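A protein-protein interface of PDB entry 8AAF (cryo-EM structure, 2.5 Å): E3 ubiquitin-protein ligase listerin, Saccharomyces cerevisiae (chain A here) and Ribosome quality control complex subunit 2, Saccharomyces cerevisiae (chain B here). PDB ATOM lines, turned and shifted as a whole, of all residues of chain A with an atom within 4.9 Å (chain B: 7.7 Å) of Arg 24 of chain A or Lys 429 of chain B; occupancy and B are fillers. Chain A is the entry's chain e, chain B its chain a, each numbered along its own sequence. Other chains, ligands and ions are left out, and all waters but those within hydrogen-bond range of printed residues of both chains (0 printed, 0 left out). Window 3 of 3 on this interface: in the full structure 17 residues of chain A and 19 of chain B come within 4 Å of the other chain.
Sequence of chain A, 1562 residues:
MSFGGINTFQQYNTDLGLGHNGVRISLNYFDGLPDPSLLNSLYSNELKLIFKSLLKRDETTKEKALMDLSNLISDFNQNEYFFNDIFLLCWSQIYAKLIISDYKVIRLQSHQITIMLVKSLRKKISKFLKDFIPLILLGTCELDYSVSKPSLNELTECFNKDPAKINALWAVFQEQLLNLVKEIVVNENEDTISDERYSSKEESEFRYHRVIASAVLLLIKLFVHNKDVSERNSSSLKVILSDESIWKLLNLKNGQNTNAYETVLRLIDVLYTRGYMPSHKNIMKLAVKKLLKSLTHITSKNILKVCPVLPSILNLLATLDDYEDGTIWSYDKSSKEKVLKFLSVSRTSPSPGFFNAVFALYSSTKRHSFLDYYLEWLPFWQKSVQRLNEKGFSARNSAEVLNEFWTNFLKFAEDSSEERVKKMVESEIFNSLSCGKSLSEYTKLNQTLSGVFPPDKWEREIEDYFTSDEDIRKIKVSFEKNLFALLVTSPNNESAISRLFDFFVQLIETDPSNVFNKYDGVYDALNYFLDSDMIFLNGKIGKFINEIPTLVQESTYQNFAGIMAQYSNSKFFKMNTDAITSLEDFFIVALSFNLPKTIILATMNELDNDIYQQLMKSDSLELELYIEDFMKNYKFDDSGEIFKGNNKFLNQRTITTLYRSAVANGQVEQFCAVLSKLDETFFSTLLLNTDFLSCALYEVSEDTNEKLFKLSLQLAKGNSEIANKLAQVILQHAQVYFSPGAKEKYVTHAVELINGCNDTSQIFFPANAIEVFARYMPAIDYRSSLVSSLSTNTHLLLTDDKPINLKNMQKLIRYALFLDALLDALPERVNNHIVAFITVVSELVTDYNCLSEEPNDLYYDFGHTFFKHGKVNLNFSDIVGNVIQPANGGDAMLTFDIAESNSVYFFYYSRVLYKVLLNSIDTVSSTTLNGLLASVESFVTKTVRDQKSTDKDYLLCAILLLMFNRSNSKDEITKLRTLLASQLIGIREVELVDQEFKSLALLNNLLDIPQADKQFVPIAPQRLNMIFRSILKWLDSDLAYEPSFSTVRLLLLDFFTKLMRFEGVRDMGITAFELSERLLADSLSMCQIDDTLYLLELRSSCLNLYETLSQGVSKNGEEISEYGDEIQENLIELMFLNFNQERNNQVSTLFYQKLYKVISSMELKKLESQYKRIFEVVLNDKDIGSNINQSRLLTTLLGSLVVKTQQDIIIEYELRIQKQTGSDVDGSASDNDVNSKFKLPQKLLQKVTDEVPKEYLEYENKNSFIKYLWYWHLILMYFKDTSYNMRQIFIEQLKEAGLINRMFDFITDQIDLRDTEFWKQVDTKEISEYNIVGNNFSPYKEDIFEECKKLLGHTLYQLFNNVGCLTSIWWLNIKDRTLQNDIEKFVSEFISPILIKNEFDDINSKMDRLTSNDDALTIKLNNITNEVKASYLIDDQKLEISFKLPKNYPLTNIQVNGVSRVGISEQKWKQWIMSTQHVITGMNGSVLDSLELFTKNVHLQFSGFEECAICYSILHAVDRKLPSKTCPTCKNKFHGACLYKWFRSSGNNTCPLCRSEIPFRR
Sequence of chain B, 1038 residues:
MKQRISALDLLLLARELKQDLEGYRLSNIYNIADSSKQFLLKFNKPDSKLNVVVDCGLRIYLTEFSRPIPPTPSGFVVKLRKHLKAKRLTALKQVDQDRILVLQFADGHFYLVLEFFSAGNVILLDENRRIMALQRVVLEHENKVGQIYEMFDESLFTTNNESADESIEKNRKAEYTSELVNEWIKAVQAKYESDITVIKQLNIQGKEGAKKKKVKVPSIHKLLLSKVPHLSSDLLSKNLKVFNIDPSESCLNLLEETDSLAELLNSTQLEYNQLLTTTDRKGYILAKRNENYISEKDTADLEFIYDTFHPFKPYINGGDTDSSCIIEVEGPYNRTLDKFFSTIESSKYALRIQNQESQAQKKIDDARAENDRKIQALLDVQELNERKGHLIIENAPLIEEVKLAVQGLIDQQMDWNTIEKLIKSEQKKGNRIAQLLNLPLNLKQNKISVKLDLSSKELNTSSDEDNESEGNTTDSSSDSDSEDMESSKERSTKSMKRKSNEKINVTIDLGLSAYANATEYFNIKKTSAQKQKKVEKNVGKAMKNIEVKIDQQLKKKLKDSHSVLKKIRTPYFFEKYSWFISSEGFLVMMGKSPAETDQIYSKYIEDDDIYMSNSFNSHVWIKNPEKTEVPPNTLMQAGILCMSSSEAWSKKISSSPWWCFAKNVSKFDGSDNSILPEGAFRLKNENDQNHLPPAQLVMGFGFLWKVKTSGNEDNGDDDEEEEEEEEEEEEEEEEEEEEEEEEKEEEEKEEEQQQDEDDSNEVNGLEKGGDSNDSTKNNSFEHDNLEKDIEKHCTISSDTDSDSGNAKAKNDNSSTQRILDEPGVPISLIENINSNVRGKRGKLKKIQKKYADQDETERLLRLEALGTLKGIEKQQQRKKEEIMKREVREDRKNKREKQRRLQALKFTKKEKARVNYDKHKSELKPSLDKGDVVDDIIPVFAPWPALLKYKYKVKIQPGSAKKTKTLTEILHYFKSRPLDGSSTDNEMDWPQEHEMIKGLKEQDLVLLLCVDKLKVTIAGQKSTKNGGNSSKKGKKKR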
ATOM      1  N   GLN A  10     -19.904   3.851   6.161  1.00  0.00           N
ATOM      2  CA  GLN A  10     -19.998   2.934   7.287  1.00  0.00           C
ATOM      3  C   GLN A  10     -21.426   2.553   7.622  1.00  0.00           C
ATOM      4  O   GLN A  10     -21.686   1.419   8.016  1.00  0.00           O
ATOM      5  CB  GLN A  10     -19.303   3.526   8.510  1.00  0.00           C
ATOM      6  CG  GLN A  10     -17.858   3.925   8.257  1.00  0.00           C
ATOM      7  CD  GLN A  10     -16.977   2.757   7.860  1.00  0.00           C
ATOM      8  OE1 GLN A  10     -17.118   1.648   8.377  1.00  0.00           O
ATOM      9  NE2 GLN A  10     -16.047   3.006   6.947  1.00  0.00           N
ATOM     10  N   ASN A  13     -22.661  -0.507   5.812  1.00  0.00           N
ATOM     11  CA  ASN A  13     -22.027  -1.785   6.158  1.00  0.00           C
ATOM     12  C   ASN A  13     -22.605  -2.524   7.360  1.00  0.00           C
ATOM     13  O   ASN A  13     -22.755  -3.744   7.309  1.00  0.00           O
ATOM     14  CB  ASN A  13     -20.529  -1.558   6.382  1.00  0.00           C
ATOM     15  CG  ASN A  13     -19.704  -2.807   6.141  1.00  0.00           C
ATOM     16  OD1 ASN A  13     -20.147  -3.740   5.472  1.00  0.00           O
ATOM     17  ND2 ASN A  13     -18.488  -2.822   6.675  1.00  0.00           N
ATOM     18  N   ASP A  15     -21.322  -3.497  10.142  1.00  0.00           N
ATOM     19  CA  ASP A  15     -20.486  -4.522  10.755  1.00  0.00           C
ATOM     20  C   ASP A  15     -19.672  -3.785  11.777  1.00  0.00           C
ATOM     21  O   ASP A  15     -18.985  -2.822  11.450  1.00  0.00           O
ATOM     22  CB  ASP A  15     -19.564  -5.171   9.735  1.00  0.00           C
ATOM     23  CG  ASP A  15     -18.719  -6.275  10.338  1.00  0.00           C
ATOM     24  OD1 ASP A  15     -19.111  -6.826  11.387  1.00  0.00           O
ATOM     25  OD2 ASP A  15     -17.664  -6.600   9.757  1.00  0.00           O
ATOM     26  N   LEU A  16     -19.730  -4.226  13.018  1.00  0.00           N
ATOM     27  CA  LEU A  16     -19.045  -3.496  14.060  1.00  0.00           C
ATOM     28  C   LEU A  16     -17.670  -4.060  14.370  1.00  0.00           C
ATOM     29  O   LEU A  16     -16.985  -3.573  15.262  1.00  0.00           O
ATOM     30  CB  LEU A  16     -19.918  -3.435  15.302  1.00  0.00           C
ATOM     31  CG  LEU A  16     -21.327  -2.899  15.080  1.00  0.00           C
ATOM     32  CD1 LEU A  16     -22.154  -3.034  16.346  1.00  0.00           C
ATOM     33  CD2 LEU A  16     -21.277  -1.457  14.604  1.00  0.00           C
ATOM     34  N   GLY A  17     -17.262  -5.091  13.645  1.00  0.00           N
ATOM     35  CA  GLY A  17     -15.954  -5.663  13.862  1.00  0.00           C
ATOM     36  C   GLY A  17     -15.837  -6.093  15.294  1.00  0.00           C
ATOM     37  O   GLY A  17     -16.701  -6.798  15.805  1.00  0.00           O
ATOM     38  N   GLY A  22     -22.078  -0.474  18.965  1.00  0.00           N
ATOM     39  CA  GLY A  22     -22.527   0.387  17.887  1.00  0.00           C
ATOM     40  C   GLY A  22     -21.459   1.189  17.187  1.00  0.00           C
ATOM     41  O   GLY A  22     -21.762   1.972  16.294  1.00  0.00           O
ATOM     42  N   VAL A  23     -20.208   1.006  17.574  1.00  0.00           N
ATOM     43  CA  VAL A  23     -19.121   1.669  16.880  1.00  0.00           C
ATOM     44  C   VAL A  23     -18.211   0.587  16.335  1.00  0.00           C
ATOM     45  O   VAL A  23     -17.892  -0.370  17.031  1.00  0.00           O
ATOM     46  CB  VAL A  23     -18.339   2.607  17.808  1.00  0.00           C
ATOM     47  CG1 VAL A  23     -19.099   3.905  18.023  1.00  0.00           C
ATOM     48  CG2 VAL A  23     -18.026   1.934  19.135  1.00  0.00           C
ATOM     49  N   ARG A  24     -17.821   0.699  15.077  1.00  0.00           N
ATOM     50  CA  ARG A  24     -16.911  -0.280  14.532  1.00  0.00           C
ATOM     51  C   ARG A  24     -15.551  -0.105  15.140  1.00  0.00           C
ATOM     52  O   ARG A  24     -15.025   0.999  15.178  1.00  0.00           O
ATOM     53  CB  ARG A  24     -16.830  -0.157  13.014  1.00  0.00           C
ATOM     54  CG  ARG A  24     -15.835  -1.102  12.371  1.00  0.00           C
ATOM     55  CD  ARG A  24     -15.979  -1.120  10.860  1.00  0.00           C
ATOM     56  NE  ARG A  24     -14.879  -1.846  10.235  1.00  0.00           N
ATOM     57  CZ  ARG A  24     -14.867  -3.157  10.027  1.00  0.00           C
ATOM     58  NH1 ARG A  24     -15.903  -3.902  10.390  1.00  0.00           N
ATOM     59  NH2 ARG A  24     -13.816  -3.726   9.456  1.00  0.00           N
ATOM     60  N   ILE A  25     -14.967  -1.188  15.618  1.00  0.00           N
ATOM     61  CA  ILE A  25     -13.630  -1.121  16.156  1.00  0.00           C
ATOM     62  C   ILE A  25     -12.836  -2.075  15.299  1.00  0.00           C
ATOM     63  O   ILE A  25     -13.188  -3.240  15.193  1.00  0.00           O
ATOM     64  CB  ILE A  25     -13.612  -1.582  17.618  1.00  0.00           C
ATOM     65  CG1 ILE A  25     -14.513  -0.701  18.474  1.00  0.00           C
ATOM     66  CG2 ILE A  25     -12.212  -1.557  18.182  1.00  0.00           C
ATOM     67  CD1 ILE A  25     -14.538  -1.122  19.921  1.00  0.00           C
ATOM     68  N   SER A  26     -11.779  -1.590  14.667  1.00  0.00           N
ATOM     69  CA  SER A  26     -10.982  -2.435  13.792  1.00  0.00           C
ATOM     70  C   SER A  26      -9.509  -2.091  13.797  1.00  0.00           C
ATOM     71  O   SER A  26      -9.145  -0.941  14.000  1.00  0.00           O
ATOM     72  CB  SER A  26     -11.507  -2.361  12.367  1.00  0.00           C
ATOM     73  OG  SER A  26     -11.342  -1.061  11.838  1.00  0.00           O
ATOM     74  N   ASN A  28      -7.362  -2.213  11.167  1.00  0.00           N
ATOM     75  CA  ASN A  28      -6.920  -1.525   9.954  1.00  0.00           C
ATOM     76  C   ASN A  28      -6.933  -0.013  10.035  1.00  0.00           C
ATOM     77  O   ASN A  28      -7.839   0.576  10.604  1.00  0.00           O
ATOM     78  CB  ASN A  28      -7.743  -1.978   8.747  1.00  0.00           C
ATOM     79  CG  ASN A  28      -9.219  -2.140   9.056  1.00  0.00           C
ATOM     80  OD1 ASN A  28      -9.731  -1.609  10.037  1.00  0.00           O
ATOM     81  ND2 ASN A  28      -9.913  -2.882   8.205  1.00  0.00           N
ATOM     82  N   ASP A  31     -10.266   2.243   8.374  1.00  0.00           N
ATOM     83  CA  ASP A  31     -11.603   2.331   8.950  1.00  0.00           C
ATOM     84  C   ASP A  31     -11.649   2.059  10.427  1.00  0.00           C
ATOM     85  O   ASP A  31     -10.709   1.515  10.984  1.00  0.00           O
ATOM     86  CB  ASP A  31     -12.610   1.451   8.198  1.00  0.00           C
ATOM     87  CG  ASP A  31     -12.332  -0.035   8.331  1.00  0.00           C
ATOM     88  OD1 ASP A  31     -12.440  -0.586   9.443  1.00  0.00           O
ATOM     89  OD2 ASP A  31     -12.052  -0.673   7.299  1.00  0.00           O
ATOM     90  N   GLY A  32     -12.749   2.427  11.066  1.00  0.00           N
ATOM     91  CA  GLY A  32     -12.859   2.270  12.501  1.00  0.00           C
ATOM     92  C   GLY A  32     -12.426   3.528  13.199  1.00  0.00           C
ATOM     93  O   GLY A  32     -12.375   3.570  14.422  1.00  0.00           O
ATOM     94  N   GLN A  93     -12.502   2.856  19.935  1.00  0.00           N
ATOM     95  CA  GLN A  93     -12.087   2.830  18.546  1.00  0.00           C
ATOM     96  C   GLN A  93     -10.618   3.148  18.334  1.00  0.00           C
ATOM     97  O   GLN A  93      -9.951   2.479  17.561  1.00  0.00           O
ATOM     98  CB  GLN A  93     -12.950   3.768  17.722  1.00  0.00           C
ATOM     99  CG  GLN A  93     -14.421   3.420  17.748  1.00  0.00           C
ATOM    100  CD  GLN A  93     -15.249   4.385  16.936  1.00  0.00           C
ATOM    101  OE1 GLN A  93     -15.646   5.440  17.425  1.00  0.00           O
ATOM    102  NE2 GLN A  93     -15.520   4.027  15.689  1.00  0.00           N
ATOM    103  N   GLU A 183     -10.523 -12.033  13.429  1.00  0.00           N
ATOM    104  CA  GLU A 183     -10.341 -10.805  12.695  1.00  0.00           C
ATOM    105  C   GLU A 183      -8.897 -10.594  12.287  1.00  0.00           C
ATOM    106  O   GLU A 183      -8.626 -10.251  11.146  1.00  0.00           O
ATOM    107  CB  GLU A 183     -10.832  -9.630  13.524  1.00  0.00           C
ATOM    108  CG  GLU A 183     -10.776  -8.290  12.819  1.00  0.00           C
ATOM    109  CD  GLU A 183     -12.016  -7.463  13.071  1.00  0.00           C
ATOM    110  OE1 GLU A 183     -13.020  -8.033  13.547  1.00  0.00           O
ATOM    111  OE2 GLU A 183     -11.989  -6.248  12.789  1.00  0.00           O
ATOM    112  N   LEU B 422     -10.194   2.544   1.601  1.00  0.00           N
ATOM    113  CA  LEU B 422     -11.527   2.334   2.151  1.00  0.00           C
ATOM    114  C   LEU B 422     -12.537   1.942   1.081  1.00  0.00           C
ATOM    115  O   LEU B 422     -13.443   1.151   1.364  1.00  0.00           O
ATOM    116  CB  LEU B 422     -11.988   3.599   2.874  1.00  0.00           C
ATOM    117  CG  LEU B 422     -13.330   3.542   3.600  1.00  0.00           C
ATOM    118  CD1 LEU B 422     -13.322   2.439   4.630  1.00  0.00           C
ATOM    119  CD2 LEU B 422     -13.637   4.865   4.252  1.00  0.00           C
ATOM    120  N   ILE B 423     -12.399   2.468  -0.134  1.00  0.00           N
ATOM    121  CA  ILE B 423     -13.283   2.056  -1.221  1.00  0.00           C
ATOM    122  C   ILE B 423     -13.004   0.611  -1.624  1.00  0.00           C
ATOM    123  O   ILE B 423     -13.938  -0.172  -1.832  1.00  0.00           O
ATOM    124  CB  ILE B 423     -13.164   3.021  -2.417  1.00  0.00           C
ATOM    125  CG1 ILE B 423     -13.627   4.418  -2.018  1.00  0.00           C
ATOM    126  CG2 ILE B 423     -14.013   2.553  -3.588  1.00  0.00           C
ATOM    127  CD1 ILE B 423     -15.061   4.476  -1.561  1.00  0.00           C
ATOM    128  N   LYS B 424     -11.720   0.233  -1.702  1.00  0.00           N
ATOM    129  CA  LYS B 424     -11.358  -1.145  -2.048  1.00  0.00           C
ATOM    130  C   LYS B 424     -11.857  -2.146  -1.013  1.00  0.00           C
ATOM    131  O   LYS B 424     -12.379  -3.211  -1.371  1.00  0.00           O
ATOM    132  CB  LYS B 424      -9.843  -1.292  -2.199  1.00  0.00           C
ATOM    133  CG  LYS B 424      -9.237  -0.493  -3.316  1.00  0.00           C
ATOM    134  CD  LYS B 424      -7.769  -0.805  -3.505  1.00  0.00           C
ATOM    135  CE  LYS B 424      -7.126   0.197  -4.448  1.00  0.00           C
ATOM    136  NZ  LYS B 424      -5.680  -0.080  -4.654  1.00  0.00           N
ATOM    137  N   SER B 425     -11.712  -1.815   0.273  1.00  0.00           N
ATOM    138  CA  SER B 425     -12.144  -2.733   1.322  1.00  0.00           C
ATOM    139  C   SER B 425     -13.659  -2.895   1.340  1.00  0.00           C
ATOM    140  O   SER B 425     -14.166  -4.004   1.530  1.00  0.00           O
ATOM    141  CB  SER B 425     -11.645  -2.251   2.677  1.00  0.00           C
ATOM    142  OG  SER B 425     -12.338  -2.888   3.732  1.00  0.00           O
ATOM    143  N   GLU B 426     -14.400  -1.810   1.120  1.00  0.00           N
ATOM    144  CA  GLU B 426     -15.853  -1.927   1.100  1.00  0.00           C
ATOM    145  C   GLU B 426     -16.354  -2.605  -0.171  1.00  0.00           C
ATOM    146  O   GLU B 426     -17.415  -3.240  -0.149  1.00  0.00           O
ATOM    147  CB  GLU B 426     -16.495  -0.553   1.281  1.00  0.00           C
ATOM    148  CG  GLU B 426     -16.295   0.045   2.662  1.00  0.00           C
ATOM    149  CD  GLU B 426     -16.961  -0.769   3.757  1.00  0.00           C
ATOM    150  OE1 GLU B 426     -18.033  -1.358   3.501  1.00  0.00           O
ATOM    151  OE2 GLU B 426     -16.409  -0.826   4.876  1.00  0.00           O
ATOM    152  N   GLN B 427     -15.613  -2.493  -1.278  1.00  0.00           N
ATOM    153  CA  GLN B 427     -15.935  -3.297  -2.455  1.00  0.00           C
ATOM    154  C   GLN B 427     -15.708  -4.780  -2.189  1.00  0.00           C
ATOM    155  O   GLN B 427     -16.480  -5.625  -2.657  1.00  0.00           O
ATOM    156  CB  GLN B 427     -15.112  -2.843  -3.659  1.00  0.00           C
ATOM    157  CG  GLN B 427     -15.585  -1.546  -4.272  1.00  0.00           C
ATOM    158  CD  GLN B 427     -14.920  -1.250  -5.597  1.00  0.00           C
ATOM    159  OE1 GLN B 427     -13.977  -1.932  -5.997  1.00  0.00           O
ATOM    160  NE2 GLN B 427     -15.411  -0.229  -6.290  1.00  0.00           N
ATOM    161  N   LYS B 428     -14.642  -5.112  -1.455  1.00  0.00           N
ATOM    162  CA  LYS B 428     -14.419  -6.505  -1.073  1.00  0.00           C
ATOM    163  C   LYS B 428     -15.485  -7.005  -0.104  1.00  0.00           C
ATOM    164  O   LYS B 428     -15.872  -8.177  -0.160  1.00  0.00           O
ATOM    165  CB  LYS B 428     -13.031  -6.672  -0.464  1.00  0.00           C
ATOM    166  CG  LYS B 428     -11.901  -6.524  -1.463  1.00  0.00           C
ATOM    167  CD  LYS B 428     -10.553  -6.705  -0.792  1.00  0.00           C
ATOM    168  CE  LYS B 428      -9.418  -6.307  -1.719  1.00  0.00           C
ATOM    169  NZ  LYS B 428      -8.098  -6.359  -1.033  1.00  0.00           N
ATOM    170  N   LYS B 429     -15.976  -6.137   0.778  1.00  0.00           N
ATOM    171  CA  LYS B 429     -17.031  -6.495   1.715  1.00  0.00           C
ATOM    172  C   LYS B 429     -18.426  -6.266   1.145  1.00  0.00           C
ATOM    173  O   LYS B 429     -19.413  -6.391   1.877  1.00  0.00           O
ATOM    174  CB  LYS B 429     -16.863  -5.725   3.025  1.00  0.00           C
ATOM    175  CG  LYS B 429     -15.535  -5.984   3.707  1.00  0.00           C
ATOM    176  CD  LYS B 429     -15.329  -5.061   4.889  1.00  0.00           C
ATOM    177  CE  LYS B 429     -13.941  -5.240   5.477  1.00  0.00           C
ATOM    178  NZ  LYS B 429     -13.535  -4.053   6.272  1.00  0.00           N
ATOM    179  N   GLY B 430     -18.523  -5.935  -0.138  1.00  0.00           N
ATOM    180  CA  GLY B 430     -19.809  -5.940  -0.818  1.00  0.00           C
ATOM    181  C   GLY B 430     -20.727  -4.783  -0.494  1.00  0.00           C
ATOM    182  O   GLY B 430     -21.933  -4.986  -0.309  1.00  0.00           O
ATOM    183  N   ASN B 431     -20.187  -3.571  -0.418  1.00  0.00           N
ATOM    184  CA  ASN B 431     -21.027  -2.388  -0.315  1.00  0.00           C
ATOM    185  C   ASN B 431     -21.335  -1.885  -1.719  1.00  0.00           C
ATOM    186  O   ASN B 431     -20.425  -1.707  -2.534  1.00  0.00           O
ATOM    187  CB  ASN B 431     -20.338  -1.306   0.515  1.00  0.00           C
ATOM    188  CG  ASN B 431     -21.290  -0.202   0.951  1.00  0.00           C
ATOM    189  OD1 ASN B 431     -22.457  -0.171   0.561  1.00  0.00           O
ATOM    190  ND2 ASN B 431     -20.791   0.705   1.779  1.00  0.00           N
ATOM    191  N   ARG B 432     -22.623  -1.665  -1.993  1.00  0.00           N
ATOM    192  CA  ARG B 432     -23.078  -1.286  -3.330  1.00  0.00           C
ATOM    193  C   ARG B 432     -22.560   0.090  -3.733  1.00  0.00           C
ATOM    194  O   ARG B 432     -22.157   0.301  -4.886  1.00  0.00           O
ATOM    195  CB  ARG B 432     -24.604  -1.318  -3.371  1.00  0.00           C
ATOM    196  CG  ARG B 432     -25.221  -1.034  -4.730  1.00  0.00           C
ATOM    197  CD  ARG B 432     -26.729  -0.690  -4.687  1.00  0.00           C
ATOM    198  NE  ARG B 432     -27.096   0.442  -3.837  1.00  0.00           N
ATOM    199  CZ  ARG B 432     -27.480   0.364  -2.568  1.00  0.00           C
ATOM    200  NH1 ARG B 432     -27.595  -0.800  -1.949  1.00  0.00           N
ATOM    201  NH2 ARG B 432     -27.765   1.482  -1.907  1.00  0.00           N
ATOM    202  N   ALA B 434     -19.842   1.553  -2.697  1.00  0.00           N
ATOM    203  CA  ALA B 434     -18.439   1.388  -3.053  1.00  0.00           C
ATOM    204  C   ALA B 434     -18.270   0.708  -4.403  1.00  0.00           C
ATOM    205  O   ALA B 434     -17.408   1.110  -5.192  1.00  0.00           O
ATOM    206  CB  ALA B 434     -17.719   0.586  -1.976  1.00  0.00           C
ATOM    207  N   GLN B 435     -19.080  -0.313  -4.690  1.00  0.00           N
ATOM    208  CA  GLN B 435     -18.915  -1.078  -5.918  1.00  0.00           C
ATOM    209  C   GLN B 435     -19.372  -0.326  -7.158  1.00  0.00           C
ATOM    210  O   GLN B 435     -19.027  -0.739  -8.270  1.00  0.00           O
ATOM    211  CB  GLN B 435     -19.660  -2.406  -5.810  1.00  0.00           C
ATOM    212  CG  GLN B 435     -18.972  -3.415  -4.910  1.00  0.00           C
ATOM    213  CD  GLN B 435     -19.760  -4.696  -4.766  1.00  0.00           C
ATOM    214  OE1 GLN B 435     -20.891  -4.800  -5.241  1.00  0.00           O
ATOM    215  NE2 GLN B 435     -19.164  -5.686  -4.115  1.00  0.00           N
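Of the printed residues of chain B, Gln 10 of chain A touches Leu 422. Of the printed residues of chain B, Asn 13 of chain A touches Glu 426. Arg 24 of chain A touches just one residue of chain B: Lys 429 (3.2 Å). Printed residues of chain A within 4 Å of Leu 422 of chain B: Gln 10 (3.6 Å) and Asp 31 (3.8 Å). Of the printed residues of chain A, Glu 426 of chain B touches Asn 13 (3.4 Å). Lys 428 of chain B touches none of the printed residues of chain A. Of chain A, only Arg 24 (3.2 Å) and Asp 31 (3.8 Å) come within 4 Å of Lys 429 of chain B.
Hydrophobic or aromatic side chains of chain B that line the printed part of chain A: Leu 422. Among the printed residues, 5 pairs touch across the chains. Among the printed residues, Asp or Glu carboxylates within 4 Å of a Lys or Arg side-chain nitrogen of the other chain: Asp 31 of chain A with Lys 429 of chain B.
Among the printed residues, pairs that only touch across the chains: Gln 10 of chain A with Leu 422 of chain B (3.6 Å) and Asp 31 of chain A with Leu 422 of chain B (3.8 Å).
The backbone carbonyl oxygen (O) of Glu 426 of chain B lies within hydrogen-bond range of the backbone NH (N) of Asn 431 of chain B (2.8 Å). The side-chain carboxylate of Asp 15 of chain A lies within salt-bridge range of the guanidinium group of Arg 24 of chain A, 3.3 Å away. The guanidinium group (NE) of Arg 24 of chain A is in salt-bridge range of the side-chain carboxylate (OD1) of Asp 31 of chain A (2.9 Å). The backbone carbonyl oxygen (O) of Arg 24 of chain A sits at hydrogen-bond distance from the side-chain amide nitrogen (NE2) of Gln 93 of chain A, at 3.1 Å. The side-chain hydroxyl (OG) of Ser 26 of chain A is in hydrogen-bond range of the side-chain carboxylate (OD1) of Asp 31 of chain A (2.7 Å). OD1 of Asn 28 of chain A sits close to OD1 of Asp 31 of chain A, at 3.0 Å.
OE2 of Glu 426 of chain B lies within hydrogen-bond range of ND2 of Asn 13 of chain A. NZ of Lys 429 of chain B is in salt-bridge range of OD2 of Asp 31 of chain A, at 3.8 Å. NH2 of Arg 24 of chain A lies close to NZ of Lys 429 of chain B (3.2 Å).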
